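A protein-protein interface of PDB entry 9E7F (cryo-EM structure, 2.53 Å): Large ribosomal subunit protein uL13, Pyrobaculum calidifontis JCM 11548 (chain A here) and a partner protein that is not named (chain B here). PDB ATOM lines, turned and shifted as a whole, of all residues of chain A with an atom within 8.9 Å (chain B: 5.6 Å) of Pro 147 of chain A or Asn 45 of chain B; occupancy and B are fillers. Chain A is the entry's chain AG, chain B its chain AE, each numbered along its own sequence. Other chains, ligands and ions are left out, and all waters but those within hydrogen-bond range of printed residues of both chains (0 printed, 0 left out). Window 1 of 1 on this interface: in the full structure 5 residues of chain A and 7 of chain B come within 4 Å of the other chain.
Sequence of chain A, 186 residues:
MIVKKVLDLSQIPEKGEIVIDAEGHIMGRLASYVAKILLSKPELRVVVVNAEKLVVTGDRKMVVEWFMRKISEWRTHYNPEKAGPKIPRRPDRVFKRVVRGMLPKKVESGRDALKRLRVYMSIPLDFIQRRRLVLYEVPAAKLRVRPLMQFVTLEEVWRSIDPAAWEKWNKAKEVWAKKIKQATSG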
ATOM      1  N   ARG A 144      26.781 -12.499 -14.171  1.00  0.00           N
ATOM      2  CA  ARG A 144      27.811 -12.954 -13.244  1.00  0.00           C
ATOM      3  C   ARG A 144      27.138 -13.509 -12.000  1.00  0.00           C
ATOM      4  O   ARG A 144      26.529 -12.762 -11.229  1.00  0.00           O
ATOM      5  CB  ARG A 144      28.755 -11.812 -12.890  1.00  0.00           C
ATOM      6  CG  ARG A 144      29.609 -12.090 -11.673  1.00  0.00           C
ATOM      7  CD  ARG A 144      30.802 -11.162 -11.612  1.00  0.00           C
ATOM      8  NE  ARG A 144      30.626 -10.122 -10.607  1.00  0.00           N
ATOM      9  CZ  ARG A 144      30.411  -8.843 -10.885  1.00  0.00           C
ATOM     10  NH1 ARG A 144      30.335  -8.411 -12.134  1.00  0.00           N
ATOM     11  NH2 ARG A 144      30.266  -7.978  -9.887  1.00  0.00           N
ATOM     12  N   VAL A 145      27.260 -14.812 -11.793  1.00  0.00           N
ATOM     13  CA  VAL A 145      26.598 -15.474 -10.676  1.00  0.00           C
ATOM     14  C   VAL A 145      27.339 -15.159  -9.386  1.00  0.00           C
ATOM     15  O   VAL A 145      28.568 -15.274  -9.314  1.00  0.00           O
ATOM     16  CB  VAL A 145      26.519 -16.988 -10.913  1.00  0.00           C
ATOM     17  CG1 VAL A 145      25.826 -17.664  -9.750  1.00  0.00           C
ATOM     18  CG2 VAL A 145      25.787 -17.268 -12.212  1.00  0.00           C
ATOM     19  N   ARG A 146      26.592 -14.754  -8.369  1.00  0.00           N
ATOM     20  CA  ARG A 146      27.100 -14.476  -7.039  1.00  0.00           C
ATOM     21  C   ARG A 146      26.229 -15.175  -6.011  1.00  0.00           C
ATOM     22  O   ARG A 146      25.052 -15.438  -6.268  1.00  0.00           O
ATOM     23  CB  ARG A 146      27.123 -12.971  -6.753  1.00  0.00           C
ATOM     24  CG  ARG A 146      28.426 -12.303  -7.113  1.00  0.00           C
ATOM     25  CD  ARG A 146      28.212 -10.864  -7.512  1.00  0.00           C
ATOM     26  NE  ARG A 146      27.236 -10.738  -8.584  1.00  0.00           N
ATOM     27  CZ  ARG A 146      26.753  -9.583  -9.016  1.00  0.00           C
ATOM     28  NH1 ARG A 146      27.116  -8.436  -8.467  1.00  0.00           N
ATOM     29  NH2 ARG A 146      25.886  -9.578 -10.024  1.00  0.00           N
ATOM     30  N   PRO A 147      26.784 -15.501  -4.848  1.00  0.00           N
ATOM     31  CA  PRO A 147      25.980 -16.162  -3.815  1.00  0.00           C
ATOM     32  C   PRO A 147      24.909 -15.231  -3.271  1.00  0.00           C
ATOM     33  O   PRO A 147      25.103 -14.019  -3.177  1.00  0.00           O
ATOM     34  CB  PRO A 147      27.005 -16.533  -2.739  1.00  0.00           C
ATOM     35  CG  PRO A 147      28.196 -15.720  -3.012  1.00  0.00           C
ATOM     36  CD  PRO A 147      28.176 -15.276  -4.432  1.00  0.00           C
ATOM     37  N   LEU A 148      23.768 -15.817  -2.914  1.00  0.00           N
ATOM     38  CA  LEU A 148      22.627 -15.113  -2.344  1.00  0.00           C
ATOM     39  C   LEU A 148      21.998 -14.118  -3.308  1.00  0.00           C
ATOM     40  O   LEU A 148      21.385 -13.140  -2.873  1.00  0.00           O
ATOM     41  CB  LEU A 148      23.008 -14.398  -1.044  1.00  0.00           C
ATOM     42  CG  LEU A 148      23.473 -15.294   0.100  1.00  0.00           C
ATOM     43  CD1 LEU A 148      23.562 -14.498   1.384  1.00  0.00           C
ATOM     44  CD2 LEU A 148      22.539 -16.470   0.258  1.00  0.00           C
ATOM     45  N   MET A 149      22.128 -14.344  -4.610  1.00  0.00           N
ATOM     46  CA  MET A 149      21.550 -13.477  -5.623  1.00  0.00           C
ATOM     47  C   MET A 149      20.298 -14.119  -6.209  1.00  0.00           C
ATOM     48  O   MET A 149      20.210 -15.340  -6.351  1.00  0.00           O
ATOM     49  CB  MET A 149      22.565 -13.190  -6.729  1.00  0.00           C
ATOM     50  CG  MET A 149      22.058 -12.305  -7.849  1.00  0.00           C
ATOM     51  SD  MET A 149      23.205 -10.980  -8.257  1.00  0.00           S
ATOM     52  CE  MET A 149      22.358 -10.229  -9.639  1.00  0.00           C
ATOM     53  N   GLN A 150      19.329 -13.278  -6.556  1.00  0.00           N
ATOM     54  CA  GLN A 150      18.010 -13.715  -6.981  1.00  0.00           C
ATOM     55  C   GLN A 150      17.814 -13.484  -8.471  1.00  0.00           C
ATOM     56  O   GLN A 150      18.178 -12.429  -8.999  1.00  0.00           O
ATOM     57  CB  GLN A 150      16.927 -12.972  -6.205  1.00  0.00           C
ATOM     58  CG  GLN A 150      16.927 -13.268  -4.733  1.00  0.00           C
ATOM     59  CD  GLN A 150      16.315 -14.606  -4.439  1.00  0.00           C
ATOM     60  OE1 GLN A 150      17.001 -15.624  -4.417  1.00  0.00           O
ATOM     61  NE2 GLN A 150      15.009 -14.619  -4.220  1.00  0.00           N
ATOM     62  N   PHE A 151      17.225 -14.470  -9.138  1.00  0.00           N
ATOM     63  CA  PHE A 151      16.884 -14.365 -10.550  1.00  0.00           C
ATOM     64  C   PHE A 151      16.069 -15.588 -10.934  1.00  0.00           C
ATOM     65  O   PHE A 151      16.059 -16.593 -10.222  1.00  0.00           O
ATOM     66  CB  PHE A 151      18.131 -14.248 -11.434  1.00  0.00           C
ATOM     67  CG  PHE A 151      18.923 -15.516 -11.538  1.00  0.00           C
ATOM     68  CD1 PHE A 151      19.750 -15.916 -10.503  1.00  0.00           C
ATOM     69  CD2 PHE A 151      18.849 -16.303 -12.671  1.00  0.00           C
ATOM     70  CE1 PHE A 151      20.479 -17.078 -10.594  1.00  0.00           C
ATOM     71  CE2 PHE A 151      19.575 -17.464 -12.767  1.00  0.00           C
ATOM     72  CZ  PHE A 151      20.392 -17.853 -11.729  1.00  0.00           C
ATOM     73  N   PHE B  26      27.875 -22.095  -7.087  1.00  0.00           N
ATOM     74  CA  PHE B  26      27.817 -21.958  -5.637  1.00  0.00           C
ATOM     75  C   PHE B  26      26.872 -22.983  -5.023  1.00  0.00           C
ATOM     76  O   PHE B  26      26.411 -22.791  -3.894  1.00  0.00           O
ATOM     77  CB  PHE B  26      27.372 -20.550  -5.237  1.00  0.00           C
ATOM     78  CG  PHE B  26      28.224 -19.462  -5.813  1.00  0.00           C
ATOM     79  CD1 PHE B  26      29.536 -19.312  -5.416  1.00  0.00           C
ATOM     80  CD2 PHE B  26      27.718 -18.598  -6.759  1.00  0.00           C
ATOM     81  CE1 PHE B  26      30.322 -18.319  -5.948  1.00  0.00           C
ATOM     82  CE2 PHE B  26      28.503 -17.604  -7.290  1.00  0.00           C
ATOM     83  CZ  PHE B  26      29.806 -17.465  -6.883  1.00  0.00           C
ATOM     84  N   ASP B  27      26.573 -24.059  -5.742  1.00  0.00           N
ATOM     85  CA  ASP B  27      25.613 -25.066  -5.321  1.00  0.00           C
ATOM     86  C   ASP B  27      26.341 -26.316  -4.854  1.00  0.00           C
ATOM     87  O   ASP B  27      27.300 -26.760  -5.490  1.00  0.00           O
ATOM     88  CB  ASP B  27      24.664 -25.421  -6.467  1.00  0.00           C
ATOM     89  CG  ASP B  27      23.498 -24.470  -6.572  1.00  0.00           C
ATOM     90  OD1 ASP B  27      23.717 -23.247  -6.490  1.00  0.00           O
ATOM     91  OD2 ASP B  27      22.358 -24.945  -6.739  1.00  0.00           O
ATOM     92  N   PHE B  43      22.596 -27.455  -0.445  1.00  0.00           N
ATOM     93  CA  PHE B  43      22.898 -26.102   0.019  1.00  0.00           C
ATOM     94  C   PHE B  43      23.112 -25.262  -1.234  1.00  0.00           C
ATOM     95  O   PHE B  43      24.227 -25.183  -1.754  1.00  0.00           O
ATOM     96  CB  PHE B  43      24.111 -26.077   0.930  1.00  0.00           C
ATOM     97  CG  PHE B  43      23.966 -26.928   2.157  1.00  0.00           C
ATOM     98  CD1 PHE B  43      24.347 -28.254   2.146  1.00  0.00           C
ATOM     99  CD2 PHE B  43      23.453 -26.397   3.323  1.00  0.00           C
ATOM    100  CE1 PHE B  43      24.213 -29.033   3.268  1.00  0.00           C
ATOM    101  CE2 PHE B  43      23.322 -27.172   4.447  1.00  0.00           C
ATOM    102  CZ  PHE B  43      23.703 -28.492   4.420  1.00  0.00           C
ATOM    103  N   LYS B  44      22.045 -24.632  -1.714  1.00  0.00           N
ATOM    104  CA  LYS B  44      22.068 -23.939  -2.990  1.00  0.00           C
ATOM    105  C   LYS B  44      22.386 -22.463  -2.818  1.00  0.00           C
ATOM    106  O   LYS B  44      21.914 -21.818  -1.878  1.00  0.00           O
ATOM    107  CB  LYS B  44      20.725 -24.090  -3.701  1.00  0.00           C
ATOM    108  CG  LYS B  44      20.178 -25.500  -3.710  1.00  0.00           C
ATOM    109  CD  LYS B  44      18.797 -25.538  -4.343  1.00  0.00           C
ATOM    110  CE  LYS B  44      17.842 -26.407  -3.544  1.00  0.00           C
ATOM    111  NZ  LYS B  44      16.515 -25.758  -3.363  1.00  0.00           N
ATOM    112  N   ASN B  45      23.182 -21.932  -3.748  1.00  0.00           N
ATOM    113  CA  ASN B  45      23.460 -20.498  -3.836  1.00  0.00           C
ATOM    114  C   ASN B  45      24.157 -19.983  -2.582  1.00  0.00           C
ATOM    115  O   ASN B  45      23.779 -18.956  -2.020  1.00  0.00           O
ATOM    116  CB  ASN B  45      22.178 -19.712  -4.102  1.00  0.00           C
ATOM    117  CG  ASN B  45      22.410 -18.501  -4.966  1.00  0.00           C
ATOM    118  OD1 ASN B  45      23.518 -18.276  -5.445  1.00  0.00           O
ATOM    119  ND2 ASN B  45      21.367 -17.711  -5.172  1.00  0.00           N
ATOM    120  N   THR B  46      25.182 -20.690  -2.149  1.00  0.00           N
ATOM    121  CA  THR B  46      25.700 -20.334  -0.846  1.00  0.00           C
ATOM    122  C   THR B  46      27.072 -19.694  -0.956  1.00  0.00           C
ATOM    123  O   THR B  46      27.928 -20.176  -1.705  1.00  0.00           O
ATOM    124  CB  THR B  46      25.801 -21.562   0.058  1.00  0.00           C
ATOM    125  OG1 THR B  46      26.407 -22.638  -0.662  1.00  0.00           O
ATOM    126  CG2 THR B  46      24.433 -21.989   0.433  1.00  0.00           C
ATOM    127  N   PRO B  47      27.308 -18.607  -0.224  1.00  0.00           N
ATOM    128  CA  PRO B  47      28.670 -18.078  -0.126  1.00  0.00           C
ATOM    129  C   PRO B  47      29.576 -18.940   0.723  1.00  0.00           C
ATOM    130  O   PRO B  47      30.802 -18.819   0.609  1.00  0.00           O
ATOM    131  CB  PRO B  47      28.461 -16.705   0.515  1.00  0.00           C
ATOM    132  CG  PRO B  47      27.240 -16.885   1.339  1.00  0.00           C
ATOM    133  CD  PRO B  47      26.359 -17.856   0.609  1.00  0.00           C
ATOM    134  N   GLU B  68      26.002 -13.102   5.410  1.00  0.00           N
ATOM    135  CA  GLU B  68      26.724 -14.282   4.955  1.00  0.00           C
ATOM    136  C   GLU B  68      27.433 -14.982   6.105  1.00  0.00           C
ATOM    137  O   GLU B  68      27.561 -16.210   6.103  1.00  0.00           O
ATOM    138  CB  GLU B  68      27.727 -13.891   3.874  1.00  0.00           C
ATOM    139  CG  GLU B  68      27.120 -13.770   2.494  1.00  0.00           C
ATOM    140  CD  GLU B  68      27.676 -12.603   1.706  1.00  0.00           C
ATOM    141  OE1 GLU B  68      27.459 -11.447   2.121  1.00  0.00           O
ATOM    142  OE2 GLU B  68      28.332 -12.842   0.671  1.00  0.00           O
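O of Arg 146 of chain A sits close to OD1 of Asn 45 of chain B (3.3 Å).
The backbone NH (N) of Leu 148 of chain A sits at hydrogen-bond distance from the backbone carbonyl oxygen (O) of Asn 45 of chain B (3.3 Å).
The backbone carbonyl oxygen (O) of Met 149 of chain A lies within hydrogen-bond range of the side-chain amide nitrogen (ND2) of Asn 45 of chain B, 2.9 Å away.
The backbone carbonyl oxygen (O) of Arg 144 of chain A is in hydrogen-bond range of the guanidinium group (NE) of Arg 146 of chain A.
The guanidinium group (NH2) of Arg 146 of chain A sits at hydrogen-bond distance from the side-chain sulfur (SD) of Met 149 of chain A, 3.5 Å away.
The backbone NH (N) of Asn 45 of chain B is in hydrogen-bond range of the backbone carbonyl oxygen (O) of Phe 26 of chain B (3.3 Å).
O of Phe 26 of chain B lies within hydrogen-bond range of N of Thr 46 of chain B (3.0 Å).
OD1 of Asp 27 of chain B is in hydrogen-bond range of N of Asn 45 of chain B (3.1 Å).
Among the printed residues, merely in contact across the chains: Val 145 of chain A with Phe 26 of chain B (3.1 Å), Arg 146 of chain A with Phe 26 of chain B (3.4 Å), Pro 147 of chain A with Phe 26 of chain B (3.7 Å), Pro 147 of chain A with Asn 45 of chain B (3.6 Å), Pro 147 of chain A with Thr 46 of chain B (3.6 Å), Pro 147 of chain A with Pro 47 of chain B (3.3 Å), Leu 148 of chain A with Pro 47 of chain B (3.9 Å) and Leu 148 of chain A with Glu 68 of chain B (3.8 Å).
Printed residues of chain B within 4 Å of Val 145 of chain A: Phe 26 (3.1 Å).
Of the printed residues of chain B, Arg 146 of chain A touches Phe 26 and Asn 45.
Of the printed residues of chain B, Pro 147 of chain A touches Phe 26 (3.7 Å), Asn 45 (3.6 Å), Thr 46 (3.6 Å) and Pro 47 (3.3 Å).
Of the printed residues of chain B, Leu 148 of chain A touches Asn 45 (3.3 Å), Pro 47 (3.9 Å) and Glu 68 (3.8 Å).
Gln 150 of chain A touches none of the printed residues of chain B.
Of the printed residues of chain A, Phe 26 of chain B touches Val 145 (3.1 Å), Arg 146 (3.4 Å) and Pro 147 (3.7 Å).
Asn 45 of chain B touches just these residues of chain A: Arg 146 (3.3 Å), Pro 147 (3.6 Å), Leu 148 (3.3 Å) and Met 149 (2.9 Å).
Of chain A, only Pro 147 (3.6 Å) comes within 4 Å of Thr 46 of chain B.
Printed residues of chain A within 4 Å of Glu 68 of chain B: Leu 148.
The nearest residue of chain B that does not touch Pro 147 of chain A is Glu 68 of chain B (4.7 Å).
The nearest printed residue of chain B that does not touch Arg 146 of chain A is Thr 46 of chain B (6.7 Å).
Of the 8 printed residues of chain B, 5 touch a printed residue of chain A.
Of the 8 printed residues of chain A, 5 touch a printed residue of chain B.
Among the printed residues, 11 pairs touch across the chains.
Among the printed residues, no Asp or Glu carboxylate lies within 4 Å of a Lys or Arg side-chain nitrogen of the other chain.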
